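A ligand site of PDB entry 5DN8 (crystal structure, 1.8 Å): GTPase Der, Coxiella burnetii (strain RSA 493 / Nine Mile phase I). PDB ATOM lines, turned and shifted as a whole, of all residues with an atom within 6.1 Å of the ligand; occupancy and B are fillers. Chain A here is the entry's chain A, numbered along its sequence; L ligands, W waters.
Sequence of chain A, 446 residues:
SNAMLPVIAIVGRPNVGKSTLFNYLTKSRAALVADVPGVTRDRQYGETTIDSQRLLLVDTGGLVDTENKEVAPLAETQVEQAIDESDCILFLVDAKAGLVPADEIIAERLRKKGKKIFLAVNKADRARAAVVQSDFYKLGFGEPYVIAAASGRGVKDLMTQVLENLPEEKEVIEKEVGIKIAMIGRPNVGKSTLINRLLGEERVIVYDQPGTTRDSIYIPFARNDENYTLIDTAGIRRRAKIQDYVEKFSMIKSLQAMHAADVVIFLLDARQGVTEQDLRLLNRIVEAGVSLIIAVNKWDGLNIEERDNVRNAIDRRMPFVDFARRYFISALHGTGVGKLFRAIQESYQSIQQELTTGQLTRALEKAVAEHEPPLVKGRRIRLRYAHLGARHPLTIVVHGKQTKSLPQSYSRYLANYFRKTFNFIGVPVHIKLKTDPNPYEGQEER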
ATOM      1  N   GLY A 185     -19.619  20.779 -30.892  1.00  0.00           N
ATOM      2  CA  GLY A 185     -19.618  22.191 -30.568  1.00  0.00           C
ATOM      3  C   GLY A 185     -19.763  23.052 -31.818  1.00  0.00           C
ATOM      4  O   GLY A 185     -19.507  22.596 -32.942  1.00  0.00           O
ATOM      5  N   ARG A 186     -20.160  24.300 -31.603  1.00  0.00           N
ATOM      6  CA  ARG A 186     -20.302  25.258 -32.714  1.00  0.00           C
ATOM      7  C   ARG A 186     -18.972  25.557 -33.352  1.00  0.00           C
ATOM      8  O   ARG A 186     -17.906  25.282 -32.775  1.00  0.00           O
ATOM      9  CB  ARG A 186     -20.834  26.599 -32.218  1.00  0.00           C
ATOM     10  CG  ARG A 186     -22.171  26.583 -31.556  1.00  0.00           C
ATOM     11  CD  ARG A 186     -22.529  27.984 -31.037  1.00  0.00           C
ATOM     12  NE  ARG A 186     -21.626  28.520 -30.000  1.00  0.00           N
ATOM     13  CZ  ARG A 186     -20.689  29.460 -30.184  1.00  0.00           C
ATOM     14  NH1 ARG A 186     -20.497  30.027 -31.379  1.00  0.00           N
ATOM     15  NH2 ARG A 186     -19.952  29.861 -29.160  1.00  0.00           N
ATOM     16  N   PRO A 187     -19.001  26.171 -34.535  1.00  0.00           N
ATOM     17  CA  PRO A 187     -17.730  26.518 -35.141  1.00  0.00           C
ATOM     18  C   PRO A 187     -16.875  27.453 -34.291  1.00  0.00           C
ATOM     19  O   PRO A 187     -17.393  28.339 -33.621  1.00  0.00           O
ATOM     20  CB  PRO A 187     -18.133  27.263 -36.416  1.00  0.00           C
ATOM     21  CG  PRO A 187     -19.471  26.718 -36.766  1.00  0.00           C
ATOM     22  CD  PRO A 187     -20.131  26.468 -35.439  1.00  0.00           C
ATOM     23  N   ASN A 188     -15.577  27.213 -34.312  1.00  0.00           N
ATOM     24  CA  ASN A 188     -14.574  28.041 -33.663  1.00  0.00           C
ATOM     25  C   ASN A 188     -14.493  27.961 -32.141  1.00  0.00           C
ATOM     26  O   ASN A 188     -13.747  28.718 -31.530  1.00  0.00           O
ATOM     27  CB  ASN A 188     -14.706  29.505 -34.142  1.00  0.00           C
ATOM     28  CG  ASN A 188     -14.444  29.656 -35.637  1.00  0.00           C
ATOM     29  OD1 ASN A 188     -13.371  29.283 -36.125  1.00  0.00           O
ATOM     30  ND2 ASN A 188     -15.401  30.190 -36.365  1.00  0.00           N
ATOM     31  N   VAL A 189     -15.209  27.013 -31.528  1.00  0.00           N
ATOM     32  CA  VAL A 189     -15.165  26.880 -30.061  1.00  0.00           C
ATOM     33  C   VAL A 189     -13.868  26.213 -29.580  1.00  0.00           C
ATOM     34  O   VAL A 189     -13.498  26.333 -28.411  1.00  0.00           O
ATOM     35  CB  VAL A 189     -16.378  26.141 -29.473  1.00  0.00           C
ATOM     36  CG1 VAL A 189     -17.676  26.906 -29.793  1.00  0.00           C
ATOM     37  CG2 VAL A 189     -16.443  24.692 -29.932  1.00  0.00           C
ATOM     38  N   GLY A 190     -13.184  25.500 -30.471  1.00  0.00           N
ATOM     39  CA  GLY A 190     -11.920  24.855 -30.154  1.00  0.00           C
ATOM     40  C   GLY A 190     -11.801  23.374 -30.368  1.00  0.00           C
ATOM     41  O   GLY A 190     -10.874  22.752 -29.840  1.00  0.00           O
ATOM     42  N   LYS A 191     -12.693  22.780 -31.168  1.00  0.00           N
ATOM     43  CA  LYS A 191     -12.672  21.323 -31.326  1.00  0.00           C
ATOM     44  C   LYS A 191     -11.370  20.755 -31.891  1.00  0.00           C
ATOM     45  O   LYS A 191     -10.800  19.815 -31.322  1.00  0.00           O
ATOM     46  CB  LYS A 191     -13.854  20.860 -32.176  1.00  0.00           C
ATOM     47  CG  LYS A 191     -15.233  21.257 -31.608  1.00  0.00           C
ATOM     48  CD  LYS A 191     -16.382  20.793 -32.491  1.00  0.00           C
ATOM     49  CE  LYS A 191     -16.357  21.422 -33.886  1.00  0.00           C
ATOM     50  NZ  LYS A 191     -16.463  22.908 -33.932  1.00  0.00           N
ATOM     51  N   SER A 192     -10.891  21.306 -33.009  1.00  0.00           N
ATOM     52  CA  SER A 192      -9.647  20.789 -33.605  1.00  0.00           C
ATOM     53  C   SER A 192      -8.473  20.986 -32.663  1.00  0.00           C
ATOM     54  O   SER A 192      -7.621  20.105 -32.519  1.00  0.00           O
ATOM     55  CB  SER A 192      -9.375  21.381 -34.997  1.00  0.00           C
ATOM     56  OG  SER A 192      -9.004  22.744 -34.949  1.00  0.00           O
ATOM     57  N   THR A 193      -8.461  22.126 -31.966  1.00  0.00           N
ATOM     58  CA  THR A 193      -7.388  22.432 -31.020  1.00  0.00           C
ATOM     59  C   THR A 193      -7.382  21.437 -29.891  1.00  0.00           C
ATOM     60  O   THR A 193      -6.309  20.963 -29.498  1.00  0.00           O
ATOM     61  CB  THR A 193      -7.518  23.868 -30.455  1.00  0.00           C
ATOM     62  OG1 THR A 193      -7.532  24.798 -31.535  1.00  0.00           O
ATOM     63  CG2 THR A 193      -6.378  24.189 -29.525  1.00  0.00           C
ATOM     64  N   LEU A 194      -8.571  21.105 -29.367  1.00  0.00           N
ATOM     65  CA  LEU A 194      -8.671  20.144 -28.277  1.00  0.00           C
ATOM     66  C   LEU A 194      -8.309  18.736 -28.745  1.00  0.00           C
ATOM     67  O   LEU A 194      -7.646  18.001 -28.023  1.00  0.00           O
ATOM     68  CB  LEU A 194     -10.077  20.161 -27.654  1.00  0.00           C
ATOM     69  CG  LEU A 194     -10.259  19.185 -26.483  1.00  0.00           C
ATOM     70  CD1 LEU A 194      -9.250  19.450 -25.368  1.00  0.00           C
ATOM     71  CD2 LEU A 194     -11.682  19.269 -25.951  1.00  0.00           C
ATOM     72  N   ILE A 236     -12.192  17.178 -39.037  1.00  0.00           N
ATOM     73  CA  ILE A 236     -11.555  18.409 -38.591  1.00  0.00           C
ATOM     74  C   ILE A 236     -10.085  18.237 -38.170  1.00  0.00           C
ATOM     75  O   ILE A 236      -9.335  19.216 -38.117  1.00  0.00           O
ATOM     76  CB  ILE A 236     -12.352  19.094 -37.460  1.00  0.00           C
ATOM     77  CG1 ILE A 236     -12.206  18.341 -36.130  1.00  0.00           C
ATOM     78  CG2 ILE A 236     -13.811  19.246 -37.878  1.00  0.00           C
ATOM     79  CD1 ILE A 236     -12.972  18.996 -35.002  1.00  0.00           C
ATOM     80  N   ARG A 239      -8.375  18.984 -41.472  1.00  0.00           N
ATOM     81  CA  ARG A 239      -8.326  20.386 -41.904  1.00  0.00           C
ATOM     82  C   ARG A 239      -7.301  21.173 -41.098  1.00  0.00           C
ATOM     83  O   ARG A 239      -6.594  22.010 -41.650  1.00  0.00           O
ATOM     84  CB  ARG A 239      -9.682  21.106 -41.829  1.00  0.00           C
ATOM     85  CG  ARG A 239     -10.191  21.397 -40.435  1.00  0.00           C
ATOM     86  CD  ARG A 239     -10.986  22.688 -40.393  1.00  0.00           C
ATOM     87  NE  ARG A 239     -11.898  22.685 -39.263  1.00  0.00           N
ATOM     88  CZ  ARG A 239     -11.629  23.104 -38.019  1.00  0.00           C
ATOM     89  NH1 ARG A 239     -10.444  23.609 -37.674  1.00  0.00           N
ATOM     90  NH2 ARG A 239     -12.585  23.027 -37.115  1.00  0.00           N
ATOM     91  N   LEU A 267     -18.105  21.305 -26.231  1.00  0.00           N
ATOM     92  CA  LEU A 267     -17.301  22.485 -25.962  1.00  0.00           C
ATOM     93  C   LEU A 267     -18.093  23.768 -26.010  1.00  0.00           C
ATOM     94  O   LEU A 267     -18.830  24.020 -26.960  1.00  0.00           O
ATOM     95  CB  LEU A 267     -16.151  22.641 -26.975  1.00  0.00           C
ATOM     96  CG  LEU A 267     -14.939  21.729 -26.869  1.00  0.00           C
ATOM     97  CD1 LEU A 267     -15.312  20.339 -27.332  1.00  0.00           C
ATOM     98  CD2 LEU A 267     -13.801  22.268 -27.739  1.00  0.00           C
ATOM     99  N   ARG A 271     -15.285  32.767 -24.067  1.00  0.00           N
ATOM    100  CA  ARG A 271     -15.228  34.174 -24.497  1.00  0.00           C
ATOM    101  C   ARG A 271     -16.590  34.616 -25.042  1.00  0.00           C
ATOM    102  O   ARG A 271     -16.884  35.817 -25.088  1.00  0.00           O
ATOM    103  CB  ARG A 271     -14.170  34.377 -25.586  1.00  0.00           C
ATOM    104  CG  ARG A 271     -12.790  33.788 -25.300  1.00  0.00           C
ATOM    105  CD  ARG A 271     -12.177  34.275 -24.020  1.00  0.00           C
ATOM    106  NE  ARG A 271     -10.828  33.719 -23.829  1.00  0.00           N
ATOM    107  CZ  ARG A 271      -9.733  34.159 -24.425  1.00  0.00           C
ATOM    108  NH1 ARG A 271      -9.798  35.169 -25.296  1.00  0.00           N
ATOM    109  NH2 ARG A 271      -8.569  33.589 -24.172  1.00  0.00           N
ATOM    110  N   ASN A 297     -14.087  25.861 -22.772  1.00  0.00           N
ATOM    111  CA  ASN A 297     -12.803  26.164 -23.375  1.00  0.00           C
ATOM    112  C   ASN A 297     -12.491  27.663 -23.464  1.00  0.00           C
ATOM    113  O   ASN A 297     -13.386  28.504 -23.288  1.00  0.00           O
ATOM    114  CB  ASN A 297     -12.774  25.501 -24.771  1.00  0.00           C
ATOM    115  CG  ASN A 297     -11.373  25.435 -25.349  1.00  0.00           C
ATOM    116  OD1 ASN A 297     -10.407  25.177 -24.644  1.00  0.00           O
ATOM    117  ND2 ASN A 297     -11.260  25.660 -26.658  1.00  0.00           N
ATOM    118  N   LYS A 298     -11.233  27.984 -23.765  1.00  0.00           N
ATOM    119  CA  LYS A 298     -10.723  29.351 -23.858  1.00  0.00           C
ATOM    120  C   LYS A 298     -10.813  30.048 -22.490  1.00  0.00           C
ATOM    121  O   LYS A 298     -10.999  31.250 -22.396  1.00  0.00           O
ATOM    122  CB  LYS A 298     -11.405  30.177 -24.964  1.00  0.00           C
ATOM    123  CG  LYS A 298     -11.564  29.439 -26.281  1.00  0.00           C
ATOM    124  CD  LYS A 298     -11.871  30.359 -27.450  1.00  0.00           C
ATOM    125  CE  LYS A 298     -12.152  29.564 -28.714  1.00  0.00           C
ATOM    126  NZ  LYS A 298     -12.559  30.467 -29.823  1.00  0.00           N
ATOM    127  N   TRP A 299     -10.598  29.273 -21.443  1.00  0.00           N
ATOM    128  CA  TRP A 299     -10.601  29.819 -20.065  1.00  0.00           C
ATOM    129  C   TRP A 299      -9.363  30.657 -19.774  1.00  0.00           C
ATOM    130  O   TRP A 299      -9.362  31.484 -18.852  1.00  0.00           O
ATOM    131  CB  TRP A 299     -10.674  28.637 -19.136  1.00  0.00           C
ATOM    132  CG  TRP A 299     -11.090  28.843 -17.726  1.00  0.00           C
ATOM    133  CD1 TRP A 299     -10.353  28.499 -16.598  1.00  0.00           C
ATOM    134  CD2 TRP A 299     -12.333  29.346 -17.244  1.00  0.00           C
ATOM    135  NE1 TRP A 299     -11.087  28.738 -15.473  1.00  0.00           N
ATOM    136  CE2 TRP A 299     -12.304  29.240 -15.832  1.00  0.00           C
ATOM    137  CE3 TRP A 299     -13.483  29.846 -17.876  1.00  0.00           C
ATOM    138  CZ2 TRP A 299     -13.377  29.650 -15.044  1.00  0.00           C
ATOM    139  CZ3 TRP A 299     -14.562  30.219 -17.072  1.00  0.00           C
ATOM    140  CH2 TRP A 299     -14.491  30.112 -15.682  1.00  0.00           C
ATOM    141  N   ASP A 300      -8.296  30.439 -20.566  1.00  0.00           N
ATOM    142  CA  ASP A 300      -7.056  31.168 -20.408  1.00  0.00           C
ATOM    143  C   ASP A 300      -7.224  32.638 -20.602  1.00  0.00           C
ATOM    144  O   ASP A 300      -8.001  33.073 -21.440  1.00  0.00           O
ATOM    145  CB  ASP A 300      -6.002  30.691 -21.399  1.00  0.00           C
ATOM    146  CG  ASP A 300      -6.499  30.722 -22.849  1.00  0.00           C
ATOM    147  OD1 ASP A 300      -7.319  29.863 -23.198  1.00  0.00           O
ATOM    148  OD2 ASP A 300      -6.048  31.587 -23.636  1.00  0.00           O
ATOM    149  N   ILE A 329     -11.070  24.592 -19.162  1.00  0.00           N
ATOM    150  CA  ILE A 329      -9.823  24.292 -19.806  1.00  0.00           C
ATOM    151  C   ILE A 329      -9.332  25.322 -20.817  1.00  0.00           C
ATOM    152  O   ILE A 329     -10.073  26.247 -21.238  1.00  0.00           O
ATOM    153  CB  ILE A 329      -9.965  22.952 -20.609  1.00  0.00           C
ATOM    154  CG1 ILE A 329     -10.897  23.120 -21.822  1.00  0.00           C
ATOM    155  CG2 ILE A 329     -10.518  21.849 -19.706  1.00  0.00           C
ATOM    156  CD1 ILE A 329     -10.793  21.982 -22.813  1.00  0.00           C
ATOM    157  N   SER A 330      -8.077  25.121 -21.201  1.00  0.00           N
ATOM    158  CA  SER A 330      -7.491  25.818 -22.334  1.00  0.00           C
ATOM    159  C   SER A 330      -6.941  24.747 -23.269  1.00  0.00           C
ATOM    160  O   SER A 330      -5.904  24.152 -23.014  1.00  0.00           O
ATOM    161  CB  SER A 330      -6.371  26.777 -21.945  1.00  0.00           C
ATOM    162  OG  SER A 330      -5.848  27.397 -23.122  1.00  0.00           O
ATOM    163  N   ALA A 331      -7.677  24.439 -24.329  1.00  0.00           N
ATOM    164  CA  ALA A 331      -7.173  23.489 -25.320  1.00  0.00           C
ATOM    165  C   ALA A 331      -5.856  24.001 -25.932  1.00  0.00           C
ATOM    166  O   ALA A 331      -4.947  23.241 -26.269  1.00  0.00           O
ATOM    167  CB  ALA A 331      -8.192  23.265 -26.396  1.00  0.00           C
ATOM    168  N   LEU A 332      -5.750  25.322 -26.062  1.00  0.00           N
ATOM    169  CA  LEU A 332      -4.570  25.947 -26.678  1.00  0.00           C
ATOM    170  C   LEU A 332      -3.309  25.790 -25.823  1.00  0.00           C
ATOM    171  O   LEU A 332      -2.252  25.457 -26.338  1.00  0.00           O
ATOM    172  CB  LEU A 332      -4.831  27.427 -26.953  1.00  0.00           C
ATOM    173  CG  LEU A 332      -3.713  28.242 -27.628  1.00  0.00           C
ATOM    174  CD1 LEU A 332      -3.438  27.681 -29.015  1.00  0.00           C
ATOM    175  CD2 LEU A 332      -4.079  29.718 -27.707  1.00  0.00           C
ATOM    176  N   HIS A 333      -3.432  26.028 -24.522  1.00  0.00           N
ATOM    177  CA  HIS A 333      -2.293  25.958 -23.618  1.00  0.00           C
ATOM    178  C   HIS A 333      -2.161  24.629 -22.885  1.00  0.00           C
ATOM    179  O   HIS A 333      -1.116  24.369 -22.258  1.00  0.00           O
ATOM    180  CB  HIS A 333      -2.317  27.156 -22.667  1.00  0.00           C
ATOM    181  CG  HIS A 333      -2.233  28.471 -23.377  1.00  0.00           C
ATOM    182  ND1 HIS A 333      -1.101  28.877 -24.043  1.00  0.00           N
ATOM    183  CD2 HIS A 333      -3.145  29.461 -23.539  1.00  0.00           C
ATOM    184  CE1 HIS A 333      -1.310  30.058 -24.588  1.00  0.00           C
ATOM    185  NE2 HIS A 333      -2.539  30.433 -24.293  1.00  0.00           N
HETATM  186  P1  LIG L   1     -13.188  24.457 -34.186  1.00  0.00           P
HETATM  187  O1  LIG L   1     -14.189  24.256 -33.041  1.00  0.00           O
HETATM  188  O2  LIG L   1     -13.843  25.233 -35.281  1.00  0.00           O
HETATM  189  O3  LIG L   1     -12.425  23.258 -34.612  1.00  0.00           O
HETATM  190  O4  LIG L   1     -12.137  25.512 -33.505  1.00  0.00           O
HETATM  191  P2  LIG L   1     -10.535  25.526 -33.593  1.00  0.00           P
HETATM  192  O5  LIG L   1      -9.828  24.434 -32.874  1.00  0.00           O
HETATM  193  O6  LIG L   1     -10.187  25.710 -35.086  1.00  0.00           O
HETATM  194  O7  LIG L   1     -10.132  26.891 -32.848  1.00  0.00           O
HETATM  195  C1  LIG L   1     -10.721  28.110 -33.286  1.00  0.00           C
HETATM  196  C2  LIG L   1      -9.883  29.303 -32.847  1.00  0.00           C
HETATM  197  O8  LIG L   1      -9.928  29.391 -31.405  1.00  0.00           O
HETATM  198  C3  LIG L   1      -8.424  29.209 -33.210  1.00  0.00           C
HETATM  199  O9  LIG L   1      -7.912  30.524 -33.478  1.00  0.00           O
HETATM  200  C4  LIG L   1      -7.790  28.692 -31.970  1.00  0.00           C
HETATM  201  O10 LIG L   1      -6.409  29.045 -31.823  1.00  0.00           O
HETATM  202  C5  LIG L   1      -8.635  29.339 -30.887  1.00  0.00           C
HETATM  203  N1  LIG L   1      -8.600  28.553 -29.658  1.00  0.00           N
HETATM  204  C6  LIG L   1      -8.917  27.227 -29.528  1.00  0.00           C
HETATM  205  N2  LIG L   1      -8.763  26.856 -28.230  1.00  0.00           N
HETATM  206  C7  LIG L   1      -8.380  27.931 -27.533  1.00  0.00           C
HETATM  207  C8  LIG L   1      -8.068  28.193 -26.129  1.00  0.00           C
HETATM  208  O11 LIG L   1      -8.124  27.273 -25.271  1.00  0.00           O
HETATM  209  N3  LIG L   1      -7.699  29.449 -25.810  1.00  0.00           N
HETATM  210  C9  LIG L   1      -7.618  30.456 -26.739  1.00  0.00           C
HETATM  211  N4  LIG L   1      -7.241  31.689 -26.354  1.00  0.00           N
HETATM  212  N5  LIG L   1      -7.897  30.289 -28.070  1.00  0.00           N
HETATM  213  C10 LIG L   1      -8.272  29.047 -28.491  1.00  0.00           C
HETATM  214  O   HOH W   1      -6.655  34.604 -27.644  1.00  0.00           O
HETATM  215  O   HOH W   2      -7.876  26.582 -35.979  1.00  0.00           O
HETATM  216  O   HOH W   3     -16.448  23.534 -36.548  1.00  0.00           O
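The side-chain hydroxyl (OG) of Ser 192 lies within hydrogen-bond range of the guanidinium group (NH1) of Arg 239 (3.2 Å).
The side-chain carboxylate (OD1) of Asp 300 sits at hydrogen-bond distance from the side-chain hydroxyl (OG) of Ser 330 (2.9 Å).
The side-chain carboxylate (OD2) of Asp 300 lies within salt-bridge range of the guanidinium group (NH2) of Arg 271, at 3.3 Å.
The side-chain amino group (NZ) of Lys 191 is in hydrogen-bond range of the backbone carbonyl oxygen (O) of Arg 186 (3.0 Å).
The backbone carbonyl oxygen of Gly 185 sits at hydrogen-bond distance from the side-chain amino group of Lys 191, at 3.2 Å.
N of Ala 331 lies within hydrogen-bond range of OD1 of Asn 297, 2.8 Å away.
OG of Ser 330 lies within hydrogen-bond range of N of His 333, 3.1 Å away.
The backbone NH (N) of Lys 298 is in hydrogen-bond range of the backbone carbonyl oxygen (O) of Ile 329 (3.3 Å).
An oxygen (O3) of the ligand is in salt-bridge range of the guanidinium group (NH2) of Arg 239, at 2.5 Å.
The side-chain carboxylate (OD1) of Asp 300 lies within hydrogen-bond range of a nitrogen (N3) of the ligand, 2.7 Å away.
The backbone NH (N) of Thr 193 lies within hydrogen-bond range of an oxygen (O5) of the ligand, 2.8 Å away.
The side-chain hydroxyl of Thr 193 is in hydrogen-bond range of an oxygen (O5) of the ligand (2.7 Å).
O1 of the ligand sits at hydrogen-bond distance from N of Lys 191, at 2.8 Å.
An oxygen (O1) of the ligand is in salt-bridge range of the side-chain amino group of Lys 191 (2.8 Å).
The backbone NH (N) of Ser 192 lies within hydrogen-bond range of an oxygen (O3) of the ligand (3.0 Å).
O5 of the ligand lies within hydrogen-bond range of OG of Ser 192.
The backbone NH (N) of Asn 188 lies within hydrogen-bond range of an oxygen (O2) of the ligand (2.8 Å).
O11 of the ligand is in hydrogen-bond range of N of Ala 331 (3.0 Å).
N of Gly 190 lies within hydrogen-bond range of O1 of the ligand.
OG of Ser 330 is in hydrogen-bond range of O11 of the ligand, 3.1 Å away.
The side-chain amide oxygen of Asn 297 sits close to an oxygen (O11) of the ligand.
The backbone NH of Leu 332 sits at hydrogen-bond distance from an oxygen (O11) of the ligand (3.2 Å).
An oxygen (O8) of the ligand lies within hydrogen-bond range of the side-chain amino group (NZ) of Lys 298, 3.3 Å away.
N of Val 189 lies within hydrogen-bond range of O1 of the ligand (3.3 Å).
Water W3 lies within hydrogen-bond range of NZ of Lys 191 (2.7 Å) and O2 of the ligand (3.4 Å).
The guanidinium group (NH2) of Arg 271 sits close to a nitrogen (N4) of the ligand, at 3.2 Å.
Arg 186 touches the ligand.
C of Pro 187 touches O2 of the ligand, 3.9 Å away.
Hydrophobic or aromatic side chains that line the ligand: Val 189 and Leu 332.
Of the 23 residues printed, 16 come within 4 Å of the ligand.
The nearest printed residue that does not touch the ligand is Ile 236 (4.3 Å).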
